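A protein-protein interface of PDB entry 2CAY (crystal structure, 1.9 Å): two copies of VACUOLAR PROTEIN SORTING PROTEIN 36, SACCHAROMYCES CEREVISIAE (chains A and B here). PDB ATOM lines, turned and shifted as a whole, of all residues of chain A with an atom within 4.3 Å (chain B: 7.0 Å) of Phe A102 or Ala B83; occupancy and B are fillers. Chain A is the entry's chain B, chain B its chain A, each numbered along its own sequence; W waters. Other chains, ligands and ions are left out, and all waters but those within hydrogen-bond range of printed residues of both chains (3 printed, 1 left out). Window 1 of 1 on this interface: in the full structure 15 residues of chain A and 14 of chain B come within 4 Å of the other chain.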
ATOM      1  N   TYR A  11      -8.000   6.007 -16.090  1.00  0.00           N
ATOM      2  CA  TYR A  11      -9.387   6.029 -15.628  1.00  0.00           C
ATOM      3  C   TYR A  11      -9.834   7.416 -15.166  1.00  0.00           C
ATOM      4  O   TYR A  11     -11.019   7.752 -15.277  1.00  0.00           O
ATOM      5  CB  TYR A  11      -9.544   5.030 -14.479  1.00  0.00           C
ATOM      6  CG  TYR A  11      -9.101   3.617 -14.844  1.00  0.00           C
ATOM      7  CD1 TYR A  11      -9.963   2.738 -15.546  1.00  0.00           C
ATOM      8  CD2 TYR A  11      -7.838   3.164 -14.487  1.00  0.00           C
ATOM      9  CE1 TYR A  11      -9.548   1.420 -15.872  1.00  0.00           C
ATOM     10  CE2 TYR A  11      -7.407   1.865 -14.816  1.00  0.00           C
ATOM     11  CZ  TYR A  11      -8.269   1.000 -15.492  1.00  0.00           C
ATOM     12  OH  TYR A  11      -7.804  -0.270 -15.801  1.00  0.00           O
ATOM     13  N   LEU A  77     -13.689  11.182 -12.392  1.00  0.00           N
ATOM     14  CA  LEU A  77     -13.959   9.827 -12.787  1.00  0.00           C
ATOM     15  C   LEU A  77     -15.413   9.774 -13.253  1.00  0.00           C
ATOM     16  O   LEU A  77     -16.312  10.240 -12.525  1.00  0.00           O
ATOM     17  CB  LEU A  77     -13.776   8.948 -11.539  1.00  0.00           C
ATOM     18  CG  LEU A  77     -13.963   7.448 -11.648  1.00  0.00           C
ATOM     19  CD1 LEU A  77     -12.717   6.836 -12.305  1.00  0.00           C
ATOM     20  CD2 LEU A  77     -14.173   6.857 -10.266  1.00  0.00           C
ATOM     21  N   ASP A  81     -18.250   4.751 -16.071  1.00  0.00           N
ATOM     22  CA  ASP A  81     -17.153   3.774 -16.165  1.00  0.00           C
ATOM     23  C   ASP A  81     -17.102   2.756 -14.990  1.00  0.00           C
ATOM     24  O   ASP A  81     -16.222   1.876 -14.966  1.00  0.00           O
ATOM     25  CB  ASP A  81     -15.804   4.495 -16.314  1.00  0.00           C
ATOM     26  CG  ASP A  81     -15.656   5.178 -17.691  1.00  0.00           C
ATOM     27  OD1 ASP A  81     -16.411   4.815 -18.617  1.00  0.00           O
ATOM     28  OD2 ASP A  81     -14.815   6.082 -17.834  1.00  0.00           O
ATOM     29  N   LEU A  82     -18.051   2.865 -14.060  1.00  0.00           N
ATOM     30  CA  LEU A  82     -18.120   2.004 -12.871  1.00  0.00           C
ATOM     31  C   LEU A  82     -19.219   0.971 -12.946  1.00  0.00           C
ATOM     32  O   LEU A  82     -20.245   1.171 -13.605  1.00  0.00           O
ATOM     33  CB  LEU A  82     -18.345   2.856 -11.605  1.00  0.00           C
ATOM     34  CG  LEU A  82     -17.309   3.928 -11.357  1.00  0.00           C
ATOM     35  CD1 LEU A  82     -17.642   4.713 -10.049  1.00  0.00           C
ATOM     36  CD2 LEU A  82     -15.892   3.289 -11.293  1.00  0.00           C
ATOM     37  N   ALA A  83     -19.026  -0.117 -12.206  1.00  0.00           N
ATOM     38  CA  ALA A  83     -19.936  -1.231 -12.189  1.00  0.00           C
ATOM     39  C   ALA A  83     -20.462  -1.537 -10.793  1.00  0.00           C
ATOM     40  O   ALA A  83     -21.637  -1.857 -10.657  1.00  0.00           O
ATOM     41  CB  ALA A  83     -19.267  -2.488 -12.813  1.00  0.00           C
ATOM     42  N   LEU A 100     -14.349   1.306  -5.550  1.00  0.00           N
ATOM     43  CA  LEU A 100     -15.107   1.401  -6.809  1.00  0.00           C
ATOM     44  C   LEU A 100     -14.478   0.485  -7.862  1.00  0.00           C
ATOM     45  O   LEU A 100     -13.264   0.551  -8.111  1.00  0.00           O
ATOM     46  CB  LEU A 100     -15.094   2.840  -7.314  1.00  0.00           C
ATOM     47  CG  LEU A 100     -15.159   3.920  -6.205  1.00  0.00           C
ATOM     48  CD1 LEU A 100     -14.656   5.262  -6.749  1.00  0.00           C
ATOM     49  CD2 LEU A 100     -16.570   4.065  -5.790  1.00  0.00           C
ATOM     50  N   PHE A 101     -15.324  -0.319  -8.484  1.00  0.00           N
ATOM     51  CA  PHE A 101     -14.927  -1.336  -9.455  1.00  0.00           C
ATOM     52  C   PHE A 101     -15.280  -0.891 -10.867  1.00  0.00           C
ATOM     53  O   PHE A 101     -16.432  -0.482 -11.129  1.00  0.00           O
ATOM     54  CB  PHE A 101     -15.631  -2.650  -9.113  1.00  0.00           C
ATOM     55  CG  PHE A 101     -15.233  -3.208  -7.773  1.00  0.00           C
ATOM     56  CD1 PHE A 101     -14.078  -3.979  -7.652  1.00  0.00           C
ATOM     57  CD2 PHE A 101     -15.980  -2.904  -6.612  1.00  0.00           C
ATOM     58  CE1 PHE A 101     -13.686  -4.519  -6.412  1.00  0.00           C
ATOM     59  CE2 PHE A 101     -15.599  -3.419  -5.343  1.00  0.00           C
ATOM     60  CZ  PHE A 101     -14.447  -4.231  -5.246  1.00  0.00           C
ATOM     61  N   PHE A 102     -14.300  -0.933 -11.770  1.00  0.00           N
ATOM     62  CA  PHE A 102     -14.549  -0.498 -13.162  1.00  0.00           C
ATOM     63  C   PHE A 102     -15.335  -1.531 -13.956  1.00  0.00           C
ATOM     64  O   PHE A 102     -15.264  -2.730 -13.666  1.00  0.00           O
ATOM     65  CB  PHE A 102     -13.228  -0.224 -13.907  1.00  0.00           C
ATOM     66  CG  PHE A 102     -12.329   0.792 -13.232  1.00  0.00           C
ATOM     67  CD1 PHE A 102     -12.696   2.151 -13.161  1.00  0.00           C
ATOM     68  CD2 PHE A 102     -11.085   0.408 -12.746  1.00  0.00           C
ATOM     69  CE1 PHE A 102     -11.831   3.108 -12.556  1.00  0.00           C
ATOM     70  CE2 PHE A 102     -10.209   1.346 -12.145  1.00  0.00           C
ATOM     71  CZ  PHE A 102     -10.606   2.704 -12.044  1.00  0.00           C
ATOM     72  N   LYS A 103     -16.085  -1.053 -14.962  1.00  0.00           N
ATOM     73  CA  LYS A 103     -16.656  -1.912 -15.979  1.00  0.00           C
ATOM     74  C   LYS A 103     -15.552  -2.599 -16.804  1.00  0.00           C
ATOM     75  O   LYS A 103     -15.669  -3.767 -17.127  1.00  0.00           O
ATOM     76  CB  LYS A 103     -17.539  -1.097 -16.938  1.00  0.00           C
ATOM     77  CG  LYS A 103     -18.819  -0.587 -16.319  1.00  0.00           C
ATOM     78  CD  LYS A 103     -19.715  -0.032 -17.419  1.00  0.00           C
ATOM     79  CE  LYS A 103     -21.021   0.483 -16.842  1.00  0.00           C
ATOM     80  NZ  LYS A 103     -21.816   1.075 -17.957  1.00  0.00           N
ATOM     81  N   ASP A 104     -14.472  -1.891 -17.092  1.00  0.00           N
ATOM     82  CA  ASP A 104     -13.513  -2.370 -18.085  1.00  0.00           C
ATOM     83  C   ASP A 104     -12.072  -2.213 -17.581  1.00  0.00           C
ATOM     84  O   ASP A 104     -11.311  -1.423 -18.125  1.00  0.00           O
ATOM     85  CB  ASP A 104     -13.786  -1.612 -19.409  1.00  0.00           C
ATOM     86  CG  ASP A 104     -12.970  -2.135 -20.611  1.00  0.00           C
ATOM     87  OD1 ASP A 104     -12.731  -3.365 -20.728  1.00  0.00           O
ATOM     88  OD2 ASP A 104     -12.590  -1.274 -21.448  1.00  0.00           O
ATOM     89  N   PRO A 105     -11.683  -2.975 -16.539  1.00  0.00           N
ATOM     90  CA  PRO A 105     -10.338  -2.824 -16.003  1.00  0.00           C
ATOM     91  C   PRO A 105      -9.283  -3.498 -16.923  1.00  0.00           C
ATOM     92  O   PRO A 105      -9.544  -4.570 -17.478  1.00  0.00           O
ATOM     93  CB  PRO A 105     -10.414  -3.551 -14.658  1.00  0.00           C
ATOM     94  CG  PRO A 105     -11.438  -4.616 -14.868  1.00  0.00           C
ATOM     95  CD  PRO A 105     -12.450  -4.008 -15.818  1.00  0.00           C
ATOM     96  N   SER A 108      -7.208  -7.019 -12.997  1.00  0.00           N
ATOM     97  CA  SER A 108      -8.164  -6.932 -11.894  1.00  0.00           C
ATOM     98  C   SER A 108      -7.458  -6.323 -10.670  1.00  0.00           C
ATOM     99  O   SER A 108      -8.074  -6.096  -9.636  1.00  0.00           O
ATOM    100  CB  SER A 108      -8.780  -8.310 -11.657  1.00  0.00           C
ATOM    101  OG  SER A 108      -7.756  -9.298 -11.708  1.00  0.00           O
ATOM    102  N   GLU A 110      -6.637  -3.251 -10.802  1.00  0.00           N
ATOM    103  CA  GLU A 110      -6.948  -1.838 -10.933  1.00  0.00           C
ATOM    104  C   GLU A 110      -8.375  -1.580 -10.509  1.00  0.00           C
ATOM    105  O   GLU A 110      -9.309  -2.142 -11.079  1.00  0.00           O
ATOM    106  CB  GLU A 110      -6.805  -1.428 -12.384  1.00  0.00           C
ATOM    107  CG  GLU A 110      -5.390  -1.672 -12.863  1.00  0.00           C
ATOM    108  CD  GLU A 110      -5.047  -0.784 -14.001  1.00  0.00           C
ATOM    109  OE1 GLU A 110      -5.446  -1.099 -15.144  1.00  0.00           O
ATOM    110  OE2 GLU A 110      -4.409   0.254 -13.731  1.00  0.00           O
ATOM    111  N   PHE A 111      -8.527  -0.738  -9.498  1.00  0.00           N
ATOM    112  CA  PHE A 111      -9.833  -0.331  -8.996  1.00  0.00           C
ATOM    113  C   PHE A 111      -9.542   0.952  -8.215  1.00  0.00           C
ATOM    114  O   PHE A 111      -8.379   1.310  -8.038  1.00  0.00           O
ATOM    115  CB  PHE A 111     -10.472  -1.437  -8.119  1.00  0.00           C
ATOM    116  CG  PHE A 111      -9.589  -1.936  -6.985  1.00  0.00           C
ATOM    117  CD1 PHE A 111      -9.599  -1.298  -5.722  1.00  0.00           C
ATOM    118  CD2 PHE A 111      -8.783  -3.079  -7.162  1.00  0.00           C
ATOM    119  CE1 PHE A 111      -8.777  -1.798  -4.658  1.00  0.00           C
ATOM    120  CE2 PHE A 111      -7.965  -3.568  -6.123  1.00  0.00           C
ATOM    121  CZ  PHE A 111      -7.963  -2.916  -4.869  1.00  0.00           C
ATOM    122  N   VAL A 112     -10.572   1.631  -7.740  1.00  0.00           N
ATOM    123  CA  VAL A 112     -10.403   2.887  -6.995  1.00  0.00           C
ATOM    124  C   VAL A 112     -10.701   2.680  -5.538  1.00  0.00           C
ATOM    125  O   VAL A 112     -11.575   1.895  -5.202  1.00  0.00           O
ATOM    126  CB  VAL A 112     -11.419   3.962  -7.474  1.00  0.00           C
ATOM    127  CG1 VAL A 112     -11.198   5.295  -6.759  1.00  0.00           C
ATOM    128  CG2 VAL A 112     -11.320   4.126  -8.939  1.00  0.00           C
ATOM    129  N   LEU B  79     -15.718 -16.257 -18.988  1.00  0.00           N
ATOM    130  CA  LEU B  79     -14.698 -15.424 -18.330  1.00  0.00           C
ATOM    131  C   LEU B  79     -14.568 -14.036 -18.974  1.00  0.00           C
ATOM    132  O   LEU B  79     -14.286 -13.052 -18.297  1.00  0.00           O
ATOM    133  CB  LEU B  79     -13.339 -16.125 -18.311  1.00  0.00           C
ATOM    134  CG  LEU B  79     -13.214 -17.408 -17.490  1.00  0.00           C
ATOM    135  CD1 LEU B  79     -11.816 -18.054 -17.767  1.00  0.00           C
ATOM    136  CD2 LEU B  79     -13.444 -17.143 -15.975  1.00  0.00           C
ATOM    137  N   ASP B  80     -14.764 -13.970 -20.285  1.00  0.00           N
ATOM    138  CA  ASP B  80     -14.752 -12.695 -21.009  1.00  0.00           C
ATOM    139  C   ASP B  80     -15.844 -11.695 -20.554  1.00  0.00           C
ATOM    140  O   ASP B  80     -15.753 -10.529 -20.865  1.00  0.00           O
ATOM    141  CB  ASP B  80     -14.882 -12.926 -22.515  1.00  0.00           C
ATOM    142  CG  ASP B  80     -14.556 -11.660 -23.317  1.00  0.00           C
ATOM    143  OD1 ASP B  80     -13.366 -11.217 -23.315  1.00  0.00           O
ATOM    144  OD2 ASP B  80     -15.502 -11.097 -23.930  1.00  0.00           O
ATOM    145  N   ASP B  81     -16.857 -12.147 -19.829  1.00  0.00           N
ATOM    146  CA  ASP B  81     -17.909 -11.244 -19.306  1.00  0.00           C
ATOM    147  C   ASP B  81     -17.602 -10.697 -17.880  1.00  0.00           C
ATOM    148  O   ASP B  81     -18.387  -9.897 -17.311  1.00  0.00           O
ATOM    149  CB  ASP B  81     -19.254 -11.955 -19.340  1.00  0.00           C
ATOM    150  CG  ASP B  81     -19.774 -12.178 -20.785  1.00  0.00           C
ATOM    151  OD1 ASP B  81     -19.241 -11.528 -21.723  1.00  0.00           O
ATOM    152  OD2 ASP B  81     -20.698 -13.006 -20.962  1.00  0.00           O
ATOM    153  N   LEU B  82     -16.464 -11.109 -17.322  1.00  0.00           N
ATOM    154  CA  LEU B  82     -16.089 -10.755 -15.954  1.00  0.00           C
ATOM    155  C   LEU B  82     -15.027  -9.668 -15.888  1.00  0.00           C
ATOM    156  O   LEU B  82     -14.139  -9.582 -16.737  1.00  0.00           O
ATOM    157  CB  LEU B  82     -15.571 -11.994 -15.189  1.00  0.00           C
ATOM    158  CG  LEU B  82     -16.482 -13.210 -15.020  1.00  0.00           C
ATOM    159  CD1 LEU B  82     -15.796 -14.244 -14.080  1.00  0.00           C
ATOM    160  CD2 LEU B  82     -17.902 -12.853 -14.491  1.00  0.00           C
ATOM    161  N   ALA B  83     -15.121  -8.840 -14.846  1.00  0.00           N
ATOM    162  CA  ALA B  83     -14.132  -7.824 -14.554  1.00  0.00           C
ATOM    163  C   ALA B  83     -13.263  -8.134 -13.340  1.00  0.00           C
ATOM    164  O   ALA B  83     -12.042  -7.827 -13.346  1.00  0.00           O
ATOM    165  CB  ALA B  83     -14.797  -6.409 -14.430  1.00  0.00           C
ATOM    166  N   TYR B  84     -13.857  -8.732 -12.294  1.00  0.00           N
ATOM    167  CA  TYR B  84     -13.096  -9.119 -11.094  1.00  0.00           C
ATOM    168  C   TYR B  84     -13.670 -10.379 -10.487  1.00  0.00           C
ATOM    169  O   TYR B  84     -14.831 -10.699 -10.675  1.00  0.00           O
ATOM    170  CB  TYR B  84     -13.163  -8.041  -9.975  1.00  0.00           C
ATOM    171  CG  TYR B  84     -12.844  -6.620 -10.371  1.00  0.00           C
ATOM    172  CD1 TYR B  84     -11.575  -6.087 -10.114  1.00  0.00           C
ATOM    173  CD2 TYR B  84     -13.806  -5.797 -10.980  1.00  0.00           C
ATOM    174  CE1 TYR B  84     -11.241  -4.764 -10.472  1.00  0.00           C
ATOM    175  CE2 TYR B  84     -13.491  -4.466 -11.352  1.00  0.00           C
ATOM    176  CZ  TYR B  84     -12.211  -3.957 -11.075  1.00  0.00           C
ATOM    177  OH  TYR B  84     -11.901  -2.663 -11.402  1.00  0.00           O
ATOM    178  N   VAL B  85     -12.839 -11.078  -9.714  1.00  0.00           N
ATOM    179  CA  VAL B  85     -13.312 -12.102  -8.805  1.00  0.00           C
ATOM    180  C   VAL B  85     -12.711 -11.776  -7.435  1.00  0.00           C
ATOM    181  O   VAL B  85     -11.591 -11.249  -7.350  1.00  0.00           O
ATOM    182  CB  VAL B  85     -13.003 -13.562  -9.289  1.00  0.00           C
ATOM    183  CG1 VAL B  85     -13.415 -13.757 -10.718  1.00  0.00           C
ATOM    184  CG2 VAL B  85     -11.526 -13.875  -9.153  1.00  0.00           C
ATOM    185  N   LEU B 100     -18.169 -13.140  -8.212  1.00  0.00           N
ATOM    186  CA  LEU B 100     -17.851 -12.765  -9.608  1.00  0.00           C
ATOM    187  C   LEU B 100     -18.535 -11.443  -9.961  1.00  0.00           C
ATOM    188  O   LEU B 100     -19.773 -11.352  -9.902  1.00  0.00           O
ATOM    189  CB  LEU B 100     -18.326 -13.868 -10.570  1.00  0.00           C
ATOM    190  CG  LEU B 100     -17.958 -15.291 -10.137  1.00  0.00           C
ATOM    191  CD1 LEU B 100     -18.511 -16.336 -11.157  1.00  0.00           C
ATOM    192  CD2 LEU B 100     -16.458 -15.418  -9.980  1.00  0.00           C
ATOM    193  N   PHE B 101     -17.719 -10.467 -10.376  1.00  0.00           N
ATOM    194  CA  PHE B 101     -18.186  -9.150 -10.844  1.00  0.00           C
ATOM    195  C   PHE B 101     -18.181  -9.076 -12.364  1.00  0.00           C
ATOM    196  O   PHE B 101     -17.148  -9.390 -12.993  1.00  0.00           O
ATOM    197  CB  PHE B 101     -17.263  -8.069 -10.303  1.00  0.00           C
ATOM    198  CG  PHE B 101     -17.507  -7.717  -8.874  1.00  0.00           C
ATOM    199  CD1 PHE B 101     -18.664  -8.131  -8.222  1.00  0.00           C
ATOM    200  CD2 PHE B 101     -16.649  -6.841  -8.224  1.00  0.00           C
ATOM    201  CE1 PHE B 101     -18.904  -7.755  -6.926  1.00  0.00           C
ATOM    202  CE2 PHE B 101     -16.898  -6.455  -6.911  1.00  0.00           C
ATOM    203  CZ  PHE B 101     -18.028  -6.926  -6.275  1.00  0.00           C
ATOM    204  N   PHE B 102     -19.327  -8.686 -12.941  1.00  0.00           N
ATOM    205  CA  PHE B 102     -19.478  -8.560 -14.404  1.00  0.00           C
ATOM    206  C   PHE B 102     -18.955  -7.230 -14.919  1.00  0.00           C
ATOM    207  O   PHE B 102     -18.951  -6.241 -14.200  1.00  0.00           O
ATOM    208  CB  PHE B 102     -20.940  -8.674 -14.827  1.00  0.00           C
ATOM    209  CG  PHE B 102     -21.567  -9.992 -14.507  1.00  0.00           C
ATOM    210  CD1 PHE B 102     -21.116 -11.152 -15.127  1.00  0.00           C
ATOM    211  CD2 PHE B 102     -22.618 -10.063 -13.605  1.00  0.00           C
ATOM    212  CE1 PHE B 102     -21.689 -12.390 -14.831  1.00  0.00           C
ATOM    213  CE2 PHE B 102     -23.215 -11.292 -13.295  1.00  0.00           C
ATOM    214  CZ  PHE B 102     -22.742 -12.455 -13.900  1.00  0.00           C
ATOM    215  N   LYS B 103     -18.556  -7.206 -16.183  1.00  0.00           N
ATOM    216  CA  LYS B 103     -18.158  -5.967 -16.840  1.00  0.00           C
ATOM    217  C   LYS B 103     -19.374  -5.037 -17.011  1.00  0.00           C
ATOM    218  O   LYS B 103     -19.249  -3.824 -16.914  1.00  0.00           O
ATOM    219  CB  LYS B 103     -17.564  -6.261 -18.223  1.00  0.00           C
ATOM    220  CG  LYS B 103     -16.197  -6.898 -18.194  1.00  0.00           C
ATOM    221  CD  LYS B 103     -15.665  -6.939 -19.614  1.00  0.00           C
ATOM    222  CE  LYS B 103     -14.266  -7.471 -19.664  1.00  0.00           C
ATOM    223  NZ  LYS B 103     -13.938  -7.721 -21.096  1.00  0.00           N
ATOM    224  N   ASP B 104     -20.541  -5.614 -17.252  1.00  0.00           N
ATOM    225  CA  ASP B 104     -21.691  -4.820 -17.721  1.00  0.00           C
ATOM    226  C   ASP B 104     -22.975  -5.247 -16.982  1.00  0.00           C
ATOM    227  O   ASP B 104     -23.891  -5.814 -17.595  1.00  0.00           O
ATOM    228  CB  ASP B 104     -21.789  -4.995 -19.256  1.00  0.00           C
ATOM    229  CG  ASP B 104     -22.809  -4.081 -19.914  1.00  0.00           C
ATOM    230  OD1 ASP B 104     -22.984  -2.927 -19.466  1.00  0.00           O
ATOM    231  OD2 ASP B 104     -23.424  -4.538 -20.916  1.00  0.00           O
ATOM    232  N   LEU B 132      -8.810 -15.461 -15.322  1.00  0.00           N
ATOM    233  CA  LEU B 132      -9.334 -14.121 -15.592  1.00  0.00           C
ATOM    234  C   LEU B 132      -8.244 -13.120 -15.985  1.00  0.00           C
ATOM    235  O   LEU B 132      -8.358 -12.431 -17.008  1.00  0.00           O
ATOM    236  CB  LEU B 132     -10.149 -13.579 -14.385  1.00  0.00           C
ATOM    237  CG  LEU B 132     -10.750 -12.186 -14.622  1.00  0.00           C
ATOM    238  CD1 LEU B 132     -11.630 -12.153 -15.885  1.00  0.00           C
ATOM    239  CD2 LEU B 132     -11.532 -11.744 -13.405  1.00  0.00           C
ATOM    240  N   GLU B 133      -7.191 -13.008 -15.182  1.00  0.00           N
ATOM    241  CA  GLU B 133      -6.113 -12.092 -15.520  1.00  0.00           C
ATOM    242  C   GLU B 133      -5.505 -12.342 -16.933  1.00  0.00           C
ATOM    243  O   GLU B 133      -5.205 -11.366 -17.645  1.00  0.00           O
ATOM    244  CB  GLU B 133      -5.034 -12.052 -14.421  1.00  0.00           C
ATOM    245  CG  GLU B 133      -4.036 -10.872 -14.577  1.00  0.00           C
ATOM    246  CD  GLU B 133      -4.576  -9.504 -14.099  1.00  0.00           C
ATOM    247  OE1 GLU B 133      -5.804  -9.320 -13.880  1.00  0.00           O
ATOM    248  OE2 GLU B 133      -3.742  -8.590 -13.948  1.00  0.00           O
ATOM    249  N   LEU B 136      -7.941 -10.662 -19.312  1.00  0.00           N
ATOM    250  CA  LEU B 136      -7.950  -9.200 -19.172  1.00  0.00           C
ATOM    251  C   LEU B 136      -6.744  -8.531 -19.786  1.00  0.00           C
ATOM    252  O   LEU B 136      -6.889  -7.503 -20.451  1.00  0.00           O
ATOM    253  CB  LEU B 136      -8.113  -8.750 -17.705  1.00  0.00           C
ATOM    254  CG  LEU B 136      -9.515  -8.969 -17.117  1.00  0.00           C
ATOM    255  CD1 LEU B 136      -9.562  -8.592 -15.611  1.00  0.00           C
ATOM    256  CD2 LEU B 136     -10.585  -8.195 -17.901  1.00  0.00           C
HETATM  257  O   HOH W   1      -8.698  -5.685 -20.171  1.00  0.00           O
HETATM  258  O   HOH W   2     -10.106 -10.428  -9.862  1.00  0.00           O
HETATM  259  O   HOH W   3     -16.975  -4.925 -12.404  1.00  0.00           O
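The backbone NH (N) of Phe A102 sits at hydrogen-bond distance from the side-chain hydroxyl (OH) of Tyr B84 (3.0 Å). OH of Tyr B84 is in hydrogen-bond range of O of Glu A110, at 2.7 Å. The side-chain carboxylate (OE1) of Glu B133 sits at hydrogen-bond distance from the backbone NH (N) of Ser A108 (2.8 Å).
O of Asp B80 is in hydrogen-bond range of NZ of Lys B103. O of Asp B81 sits at hydrogen-bond distance from N of Lys B103 (2.9 Å). The backbone NH (N) of Ala B83 is in hydrogen-bond range of the backbone carbonyl oxygen (O) of Phe B101 (2.8 Å). N of Phe B101 lies within hydrogen-bond range of O of Tyr B84, at 2.9 Å. The side-chain carboxylate (OE1) of Glu A110 is in hydrogen-bond range of the side-chain hydroxyl (OH) of Tyr A11 (2.6 Å). The backbone NH (N) of Ala A83 sits at hydrogen-bond distance from the backbone carbonyl oxygen (O) of Phe A101.
Among the printed residues, merely in contact across the chains: Phe A101 with Tyr B84 (3.6 Å), Phe A101 with Phe B101 (3.7 Å), Phe A102 with Ala B83 (3.8 Å), Lys A103 with Ala B83 (3.9 Å), Lys A103 with Lys B103 (3.2 Å), Pro A105 with Ala B83 (3.6 Å), Pro A105 with Tyr B84 (3.7 Å), Pro A105 with Leu B136 (3.8 Å), Ser A108 with Ala B83 (3.7 Å), Ser A108 with Tyr B84 (3.5 Å), Ser A108 with Leu B136 (3.9 Å) and Phe A111 with Tyr B84 (3.8 Å).
Phe A102 touches two residues of chain B. Of chain A, only Phe A102, Lys A103, Pro A105 and Ser A108 come within 4 Å of Ala B83. Printed residues of chain A within 4 Å of Phe B101: Phe A101. Printed residues of chain B within 4 Å of Pro A105: Ala B83 (3.6 Å), Tyr B84 (3.7 Å) and Leu B136 (3.8 Å). Of the printed residues of chain B, Lys A103 touches Ala B83 (3.9 Å) and Lys B103 (3.2 Å). Of the printed residues of chain B, Phe A101 touches Tyr B84 and Phe B101. Phe B102 touches none of the printed residues of chain A. The nearest residue of chain B that does not touch Phe A102 is Phe B102 (5.1 Å). The nearest printed residue of chain A that does not touch Ala B83 is Asp A104 (5.3 Å). The nearest printed residue of chain B that does not touch Glu A110 is Ala B83 (6.7 Å).
Of the 15 printed residues of chain B, 6 touch a printed residue of chain A. Printed residues of chain B that touch a printed residue of chain A: Ala B83, Tyr B84, Phe B101, Lys B103, Glu B133 and Leu B136. Among the printed residues, 15 pairs touch across the chains. Among the printed residues, no Asp or Glu carboxylate lies within 4 Å of a Lys or Arg side-chain nitrogen of the other chain.
Phe A101 touches its own counterpart, Phe B101. Phe A102 touches Ala B83, but with the chains exchanged Ala A83 does not touch Phe B102 (4.01 Å). Lys A103 touches Ala B83, but with the chains exchanged Ala A83 does not touch Lys B103 (4.3 Å). Lys B103 touches its own counterpart, Lys A103. Positions printed for both chains: 81, 82, 83, 100, 101, 102, 103 and 104. Of the 15 pairs that touch across the chains among the printed residues, 2 have their exchanged pair printed and touching as well.
Water W1 bridges O of Leu B136 (2.6 Å) and O of Pro A105 (3.0 Å). Water W2 bridges the backbone NH of Val B85 (2.8 Å) and the side-chain hydroxyl of Ser A108 (3.2 Å). Water W3 bridges O of Phe B102 (3.0 Å) and O of Phe A102 (3.1 Å).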
